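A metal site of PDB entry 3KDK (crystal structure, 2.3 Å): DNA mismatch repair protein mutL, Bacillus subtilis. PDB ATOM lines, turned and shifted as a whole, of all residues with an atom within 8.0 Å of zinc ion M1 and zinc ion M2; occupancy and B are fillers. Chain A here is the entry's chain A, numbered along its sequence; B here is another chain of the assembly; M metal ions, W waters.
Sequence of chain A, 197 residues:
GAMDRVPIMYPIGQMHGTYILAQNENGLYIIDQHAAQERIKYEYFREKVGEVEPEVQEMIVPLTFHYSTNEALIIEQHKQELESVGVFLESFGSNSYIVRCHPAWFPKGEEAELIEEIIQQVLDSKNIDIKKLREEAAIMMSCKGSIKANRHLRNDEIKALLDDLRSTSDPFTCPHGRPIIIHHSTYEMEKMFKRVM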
ATOM      1  N   ASP A  32     -23.621  -7.717  -3.407  1.00  0.00           N
ATOM      2  CA  ASP A  32     -23.609  -7.226  -2.043  1.00  0.00           C
ATOM      3  C   ASP A  32     -22.652  -8.097  -1.248  1.00  0.00           C
ATOM      4  O   ASP A  32     -22.949  -9.260  -0.959  1.00  0.00           O
ATOM      5  CB  ASP A  32     -25.019  -7.289  -1.446  1.00  0.00           C
ATOM      6  CG  ASP A  32     -25.108  -6.612  -0.089  1.00  0.00           C
ATOM      7  OD1 ASP A  32     -24.435  -7.084   0.846  1.00  0.00           O
ATOM      8  OD2 ASP A  32     -25.832  -5.604   0.024  1.00  0.00           O
ATOM      9  N   HIS A  34     -21.469  -8.123   1.818  1.00  0.00           N
ATOM     10  CA  HIS A  34     -21.866  -8.579   3.143  1.00  0.00           C
ATOM     11  C   HIS A  34     -22.882  -9.721   3.069  1.00  0.00           C
ATOM     12  O   HIS A  34     -22.740 -10.730   3.772  1.00  0.00           O
ATOM     13  CB  HIS A  34     -22.448  -7.445   3.980  1.00  0.00           C
ATOM     14  CG  HIS A  34     -22.808  -7.868   5.371  1.00  0.00           C
ATOM     15  ND1 HIS A  34     -21.920  -7.805   6.416  1.00  0.00           N
ATOM     16  CD2 HIS A  34     -23.943  -8.403   5.862  1.00  0.00           C
ATOM     17  CE1 HIS A  34     -22.503  -8.261   7.511  1.00  0.00           C
ATOM     18  NE2 HIS A  34     -23.732  -8.629   7.204  1.00  0.00           N
ATOM     19  N   ALA A  35     -23.907  -9.560   2.242  1.00  0.00           N
ATOM     20  CA  ALA A  35     -24.894 -10.610   2.020  1.00  0.00           C
ATOM     21  C   ALA A  35     -24.212 -11.885   1.538  1.00  0.00           C
ATOM     22  O   ALA A  35     -24.589 -12.998   1.927  1.00  0.00           O
ATOM     23  CB  ALA A  35     -25.950 -10.152   1.014  1.00  0.00           C
ATOM     24  N   ALA A  36     -23.205 -11.719   0.674  1.00  0.00           N
ATOM     25  CA  ALA A  36     -22.444 -12.859   0.149  1.00  0.00           C
ATOM     26  C   ALA A  36     -21.713 -13.570   1.273  1.00  0.00           C
ATOM     27  O   ALA A  36     -21.778 -14.796   1.388  1.00  0.00           O
ATOM     28  CB  ALA A  36     -21.454 -12.398  -0.913  1.00  0.00           C
ATOM     29  N   GLN A  37     -21.020 -12.807   2.099  1.00  0.00           N
ATOM     30  CA  GLN A  37     -20.277 -13.361   3.235  1.00  0.00           C
ATOM     31  C   GLN A  37     -21.208 -14.106   4.209  1.00  0.00           C
ATOM     32  O   GLN A  37     -20.820 -15.132   4.770  1.00  0.00           O
ATOM     33  CB  GLN A  37     -19.494 -12.256   3.949  1.00  0.00           C
ATOM     34  CG  GLN A  37     -18.366 -11.674   3.103  1.00  0.00           C
ATOM     35  CD  GLN A  37     -17.838 -10.357   3.647  1.00  0.00           C
ATOM     36  OE1 GLN A  37     -18.490  -9.681   4.436  1.00  0.00           O
ATOM     37  NE2 GLN A  37     -16.629  -9.981   3.219  1.00  0.00           N
ATOM     38  N   GLU A  38     -22.426 -13.601   4.380  1.00  0.00           N
ATOM     39  CA  GLU A  38     -23.432 -14.279   5.197  1.00  0.00           C
ATOM     40  C   GLU A  38     -23.772 -15.659   4.661  1.00  0.00           C
ATOM     41  O   GLU A  38     -23.783 -16.649   5.396  1.00  0.00           O
ATOM     42  CB  GLU A  38     -24.728 -13.460   5.246  1.00  0.00           C
ATOM     43  CG  GLU A  38     -24.709 -12.228   6.105  1.00  0.00           C
ATOM     44  CD  GLU A  38     -26.098 -11.639   6.245  1.00  0.00           C
ATOM     45  OE1 GLU A  38     -26.270 -10.649   6.991  1.00  0.00           O
ATOM     46  OE2 GLU A  38     -27.027 -12.183   5.614  1.00  0.00           O
ATOM     47  N   ARG A  39     -24.095 -15.718   3.369  1.00  0.00           N
ATOM     48  CA  ARG A  39     -24.453 -16.976   2.727  1.00  0.00           C
ATOM     49  C   ARG A  39     -23.335 -17.991   2.903  1.00  0.00           C
ATOM     50  O   ARG A  39     -23.573 -19.128   3.322  1.00  0.00           O
ATOM     51  CB  ARG A  39     -24.727 -16.753   1.231  1.00  0.00           C
ATOM     52  CG  ARG A  39     -24.652 -18.033   0.425  1.00  0.00           C
ATOM     53  CD  ARG A  39     -25.642 -19.075   0.924  1.00  0.00           C
ATOM     54  NE  ARG A  39     -26.999 -18.553   0.955  1.00  0.00           N
ATOM     55  CZ  ARG A  39     -28.041 -19.218   1.453  1.00  0.00           C
ATOM     56  NH1 ARG A  39     -27.887 -20.434   1.940  1.00  0.00           N
ATOM     57  NH2 ARG A  39     -29.252 -18.660   1.441  1.00  0.00           N
ATOM     58  N   ILE A 139     -27.142 -19.305  11.636  1.00  0.00           N
ATOM     59  CA  ILE A 139     -27.338 -17.915  11.258  1.00  0.00           C
ATOM     60  C   ILE A 139     -26.573 -16.975  12.186  1.00  0.00           C
ATOM     61  O   ILE A 139     -25.911 -16.033  11.736  1.00  0.00           O
ATOM     62  CB  ILE A 139     -28.831 -17.528  11.300  1.00  0.00           C
ATOM     63  CG1 ILE A 139     -29.587 -18.208  10.161  1.00  0.00           C
ATOM     64  CG2 ILE A 139     -28.989 -16.018  11.215  1.00  0.00           C
ATOM     65  CD1 ILE A 139     -31.078 -17.919  10.150  1.00  0.00           C
ATOM     66  N   SER A 142     -22.844 -16.777  11.506  1.00  0.00           N
ATOM     67  CA  SER A 142     -22.444 -16.243  10.208  1.00  0.00           C
ATOM     68  C   SER A 142     -22.347 -14.719  10.211  1.00  0.00           C
ATOM     69  O   SER A 142     -21.608 -14.128   9.422  1.00  0.00           O
ATOM     70  CB  SER A 142     -23.397 -16.718   9.116  1.00  0.00           C
ATOM     71  OG  SER A 142     -24.738 -16.433   9.457  1.00  0.00           O
ATOM     72  N   CYS A 143     -23.097 -14.067  11.103  1.00  0.00           N
ATOM     73  CA  CYS A 143     -23.002 -12.626  11.284  1.00  0.00           C
ATOM     74  C   CYS A 143     -22.093 -12.330  12.459  1.00  0.00           C
ATOM     75  O   CYS A 143     -21.966 -11.186  12.890  1.00  0.00           O
ATOM     76  CB  CYS A 143     -24.385 -12.026  11.514  1.00  0.00           C
ATOM     77  SG  CYS A 143     -25.529 -12.280  10.140  1.00  0.00           S
ATOM     78  N   LYS A 144     -21.464 -13.378  12.981  1.00  0.00           N
ATOM     79  CA  LYS A 144     -20.581 -13.280  14.132  1.00  0.00           C
ATOM     80  C   LYS A 144     -19.117 -13.209  13.688  1.00  0.00           C
ATOM     81  O   LYS A 144     -18.665 -12.199  13.157  1.00  0.00           O
ATOM     82  CB  LYS A 144     -20.783 -14.474  15.061  1.00  0.00           C
ATOM     83  CG  LYS A 144     -20.660 -14.148  16.541  1.00  0.00           C
ATOM     84  CD  LYS A 144     -22.030 -14.101  17.221  1.00  0.00           C
ATOM     85  CE  LYS A 144     -22.923 -13.049  16.598  1.00  0.00           C
ATOM     86  NZ  LYS A 144     -24.302 -13.077  17.159  1.00  0.00           N
ATOM     87  N   THR A 173     -29.351 -15.486  -2.963  1.00  0.00           N
ATOM     88  CA  THR A 173     -30.154 -15.044  -1.830  1.00  0.00           C
ATOM     89  C   THR A 173     -29.455 -15.376  -0.524  1.00  0.00           C
ATOM     90  O   THR A 173     -28.911 -16.471  -0.372  1.00  0.00           O
ATOM     91  CB  THR A 173     -31.559 -15.717  -1.872  1.00  0.00           C
ATOM     92  OG1 THR A 173     -32.153 -15.511  -3.161  1.00  0.00           O
ATOM     93  CG2 THR A 173     -32.466 -15.156  -0.795  1.00  0.00           C
ATOM     94  N   CYS A 174     -29.442 -14.427   0.419  1.00  0.00           N
ATOM     95  CA  CYS A 174     -28.848 -14.680   1.727  1.00  0.00           C
ATOM     96  C   CYS A 174     -29.840 -15.402   2.644  1.00  0.00           C
ATOM     97  O   CYS A 174     -31.033 -15.458   2.341  1.00  0.00           O
ATOM     98  CB  CYS A 174     -28.360 -13.379   2.375  1.00  0.00           C
ATOM     99  SG  CYS A 174     -29.678 -12.438   3.153  1.00  0.00           S
ATOM    100  N   PRO A 175     -29.339 -15.968   3.764  1.00  0.00           N
ATOM    101  CA  PRO A 175     -30.197 -16.770   4.650  1.00  0.00           C
ATOM    102  C   PRO A 175     -31.375 -15.979   5.217  1.00  0.00           C
ATOM    103  O   PRO A 175     -32.286 -16.566   5.785  1.00  0.00           O
ATOM    104  CB  PRO A 175     -29.242 -17.169   5.773  1.00  0.00           C
ATOM    105  CG  PRO A 175     -27.876 -17.063   5.177  1.00  0.00           C
ATOM    106  CD  PRO A 175     -27.955 -15.901   4.234  1.00  0.00           C
ATOM    107  N   HIS A 176     -31.346 -14.658   5.052  1.00  0.00           N
ATOM    108  CA  HIS A 176     -32.432 -13.813   5.520  1.00  0.00           C
ATOM    109  C   HIS A 176     -33.440 -13.483   4.418  1.00  0.00           C
ATOM    110  O   HIS A 176     -34.452 -12.828   4.669  1.00  0.00           O
ATOM    111  CB  HIS A 176     -31.885 -12.522   6.141  1.00  0.00           C
ATOM    112  CG  HIS A 176     -30.922 -12.753   7.264  1.00  0.00           C
ATOM    113  ND1 HIS A 176     -29.566 -12.861   7.074  1.00  0.00           N
ATOM    114  CD2 HIS A 176     -31.125 -12.900   8.598  1.00  0.00           C
ATOM    115  CE1 HIS A 176     -28.966 -13.055   8.229  1.00  0.00           C
ATOM    116  NE2 HIS A 176     -29.894 -13.092   9.172  1.00  0.00           N
ATOM    117  N   GLY A 177     -33.172 -13.931   3.197  1.00  0.00           N
ATOM    118  CA  GLY A 177     -34.099 -13.749   2.095  1.00  0.00           C
ATOM    119  C   GLY A 177     -33.785 -12.591   1.155  1.00  0.00           C
ATOM    120  O   GLY A 177     -34.463 -12.402   0.151  1.00  0.00           O
ATOM    121  N   ARG A 178     -32.763 -11.813   1.491  1.00  0.00           N
ATOM    122  CA  ARG A 178     -32.368 -10.668   0.678  1.00  0.00           C
ATOM    123  C   ARG A 178     -31.431 -11.049  -0.472  1.00  0.00           C
ATOM    124  O   ARG A 178     -30.635 -11.973  -0.354  1.00  0.00           O
ATOM    125  CB  ARG A 178     -31.725  -9.583   1.555  1.00  0.00           C
ATOM    126  CG  ARG A 178     -32.745  -8.752   2.313  1.00  0.00           C
ATOM    127  CD  ARG A 178     -32.146  -7.989   3.482  1.00  0.00           C
ATOM    128  NE  ARG A 178     -33.009  -8.075   4.651  1.00  0.00           N
ATOM    129  CZ  ARG A 178     -32.681  -8.687   5.784  1.00  0.00           C
ATOM    130  NH1 ARG A 178     -33.536  -8.727   6.802  1.00  0.00           N
ATOM    131  NH2 ARG A 178     -31.482  -9.253   5.918  1.00  0.00           N
ATOM    132  N   PRO A 179     -31.547 -10.331  -1.608  1.00  0.00           N
ATOM    133  CA  PRO A 179     -30.767 -10.629  -2.809  1.00  0.00           C
ATOM    134  C   PRO A 179     -29.280 -10.437  -2.563  1.00  0.00           C
ATOM    135  O   PRO A 179     -28.891  -9.467  -1.927  1.00  0.00           O
ATOM    136  CB  PRO A 179     -31.264  -9.584  -3.825  1.00  0.00           C
ATOM    137  CG  PRO A 179     -32.582  -9.134  -3.290  1.00  0.00           C
ATOM    138  CD  PRO A 179     -32.443  -9.183  -1.801  1.00  0.00           C
ATOM    139  N   ILE A 180     -28.460 -11.364  -3.054  1.00  0.00           N
ATOM    140  CA  ILE A 180     -27.011 -11.249  -2.988  1.00  0.00           C
ATOM    141  C   ILE A 180     -26.460 -10.719  -4.321  1.00  0.00           C
ATOM    142  O   ILE A 180     -25.483  -9.967  -4.349  1.00  0.00           O
ATOM    143  CB  ILE A 180     -26.341 -12.604  -2.703  1.00  0.00           C
ATOM    144  CG1 ILE A 180     -26.704 -13.098  -1.299  1.00  0.00           C
ATOM    145  CG2 ILE A 180     -24.820 -12.485  -2.828  1.00  0.00           C
ATOM    146  CD1 ILE A 180     -26.227 -14.498  -1.011  1.00  0.00           C
ATOM    147  N   PHE B 193     -31.172  -4.357  -3.314  1.00  0.00           N
ATOM    148  CA  PHE B 193     -30.644  -5.410  -2.438  1.00  0.00           C
ATOM    149  C   PHE B 193     -31.421  -5.639  -1.138  1.00  0.00           C
ATOM    150  O   PHE B 193     -31.110  -6.578  -0.403  1.00  0.00           O
ATOM    151  CB  PHE B 193     -29.175  -5.154  -2.113  1.00  0.00           C
ATOM    152  CG  PHE B 193     -28.244  -5.403  -3.257  1.00  0.00           C
ATOM    153  CD1 PHE B 193     -27.861  -6.697  -3.593  1.00  0.00           C
ATOM    154  CD2 PHE B 193     -27.728  -4.350  -3.998  1.00  0.00           C
ATOM    155  CE1 PHE B 193     -26.997  -6.933  -4.651  1.00  0.00           C
ATOM    156  CE2 PHE B 193     -26.858  -4.578  -5.057  1.00  0.00           C
ATOM    157  CZ  PHE B 193     -26.497  -5.866  -5.384  1.00  0.00           C
HETATM  158 ZN    ZN M   1     -29.028 -11.285   5.249  1.00  0.00          ZN
HETATM  159 ZN    ZN M   2     -25.148  -9.758   8.703  1.00  0.00          ZN
HETATM  160  O   HOH W   1     -28.890  -9.083   6.205  1.00  0.00           O
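OE1 of Glu 38 binds zinc ion M2 (2.2 Å).
Zinc ion M2 is bound by a ring nitrogen (NE2) of His 34 (2.4 Å).
Zinc ion M2 has two donor atoms within binding distance.
Slightly farther from zinc ion M2 lies the side-chain sulfur (SG) of Cys 143 (2.9 Å).
Arg 178 touches zinc ion M1.
Four residues have an atom within 4 Å of zinc ion M1: Glu 38, Cys 174, His 176 and Arg 178.
The nearest printed residue that does not touch zinc ion M2 is His 176 (5.1 Å).
Zinc ion M1 is bound by the side-chain carboxylate of Glu 38 (2.2 Å), water W1 (2.4 Å), a ring nitrogen (ND1) of His 176 (2.5 Å) and the side-chain sulfur of Cys 174 (2.5 Å).
SG of Cys 143 sits close to OE1 of Glu 38 (3.6 Å).
The backbone NH (N) of His 34 sits close to the side-chain carboxylate (OD1) of Asp 32, at 3.3 Å.
The backbone NH (N) of Arg 178 sits close to the side-chain sulfur (SG) of Cys 174.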
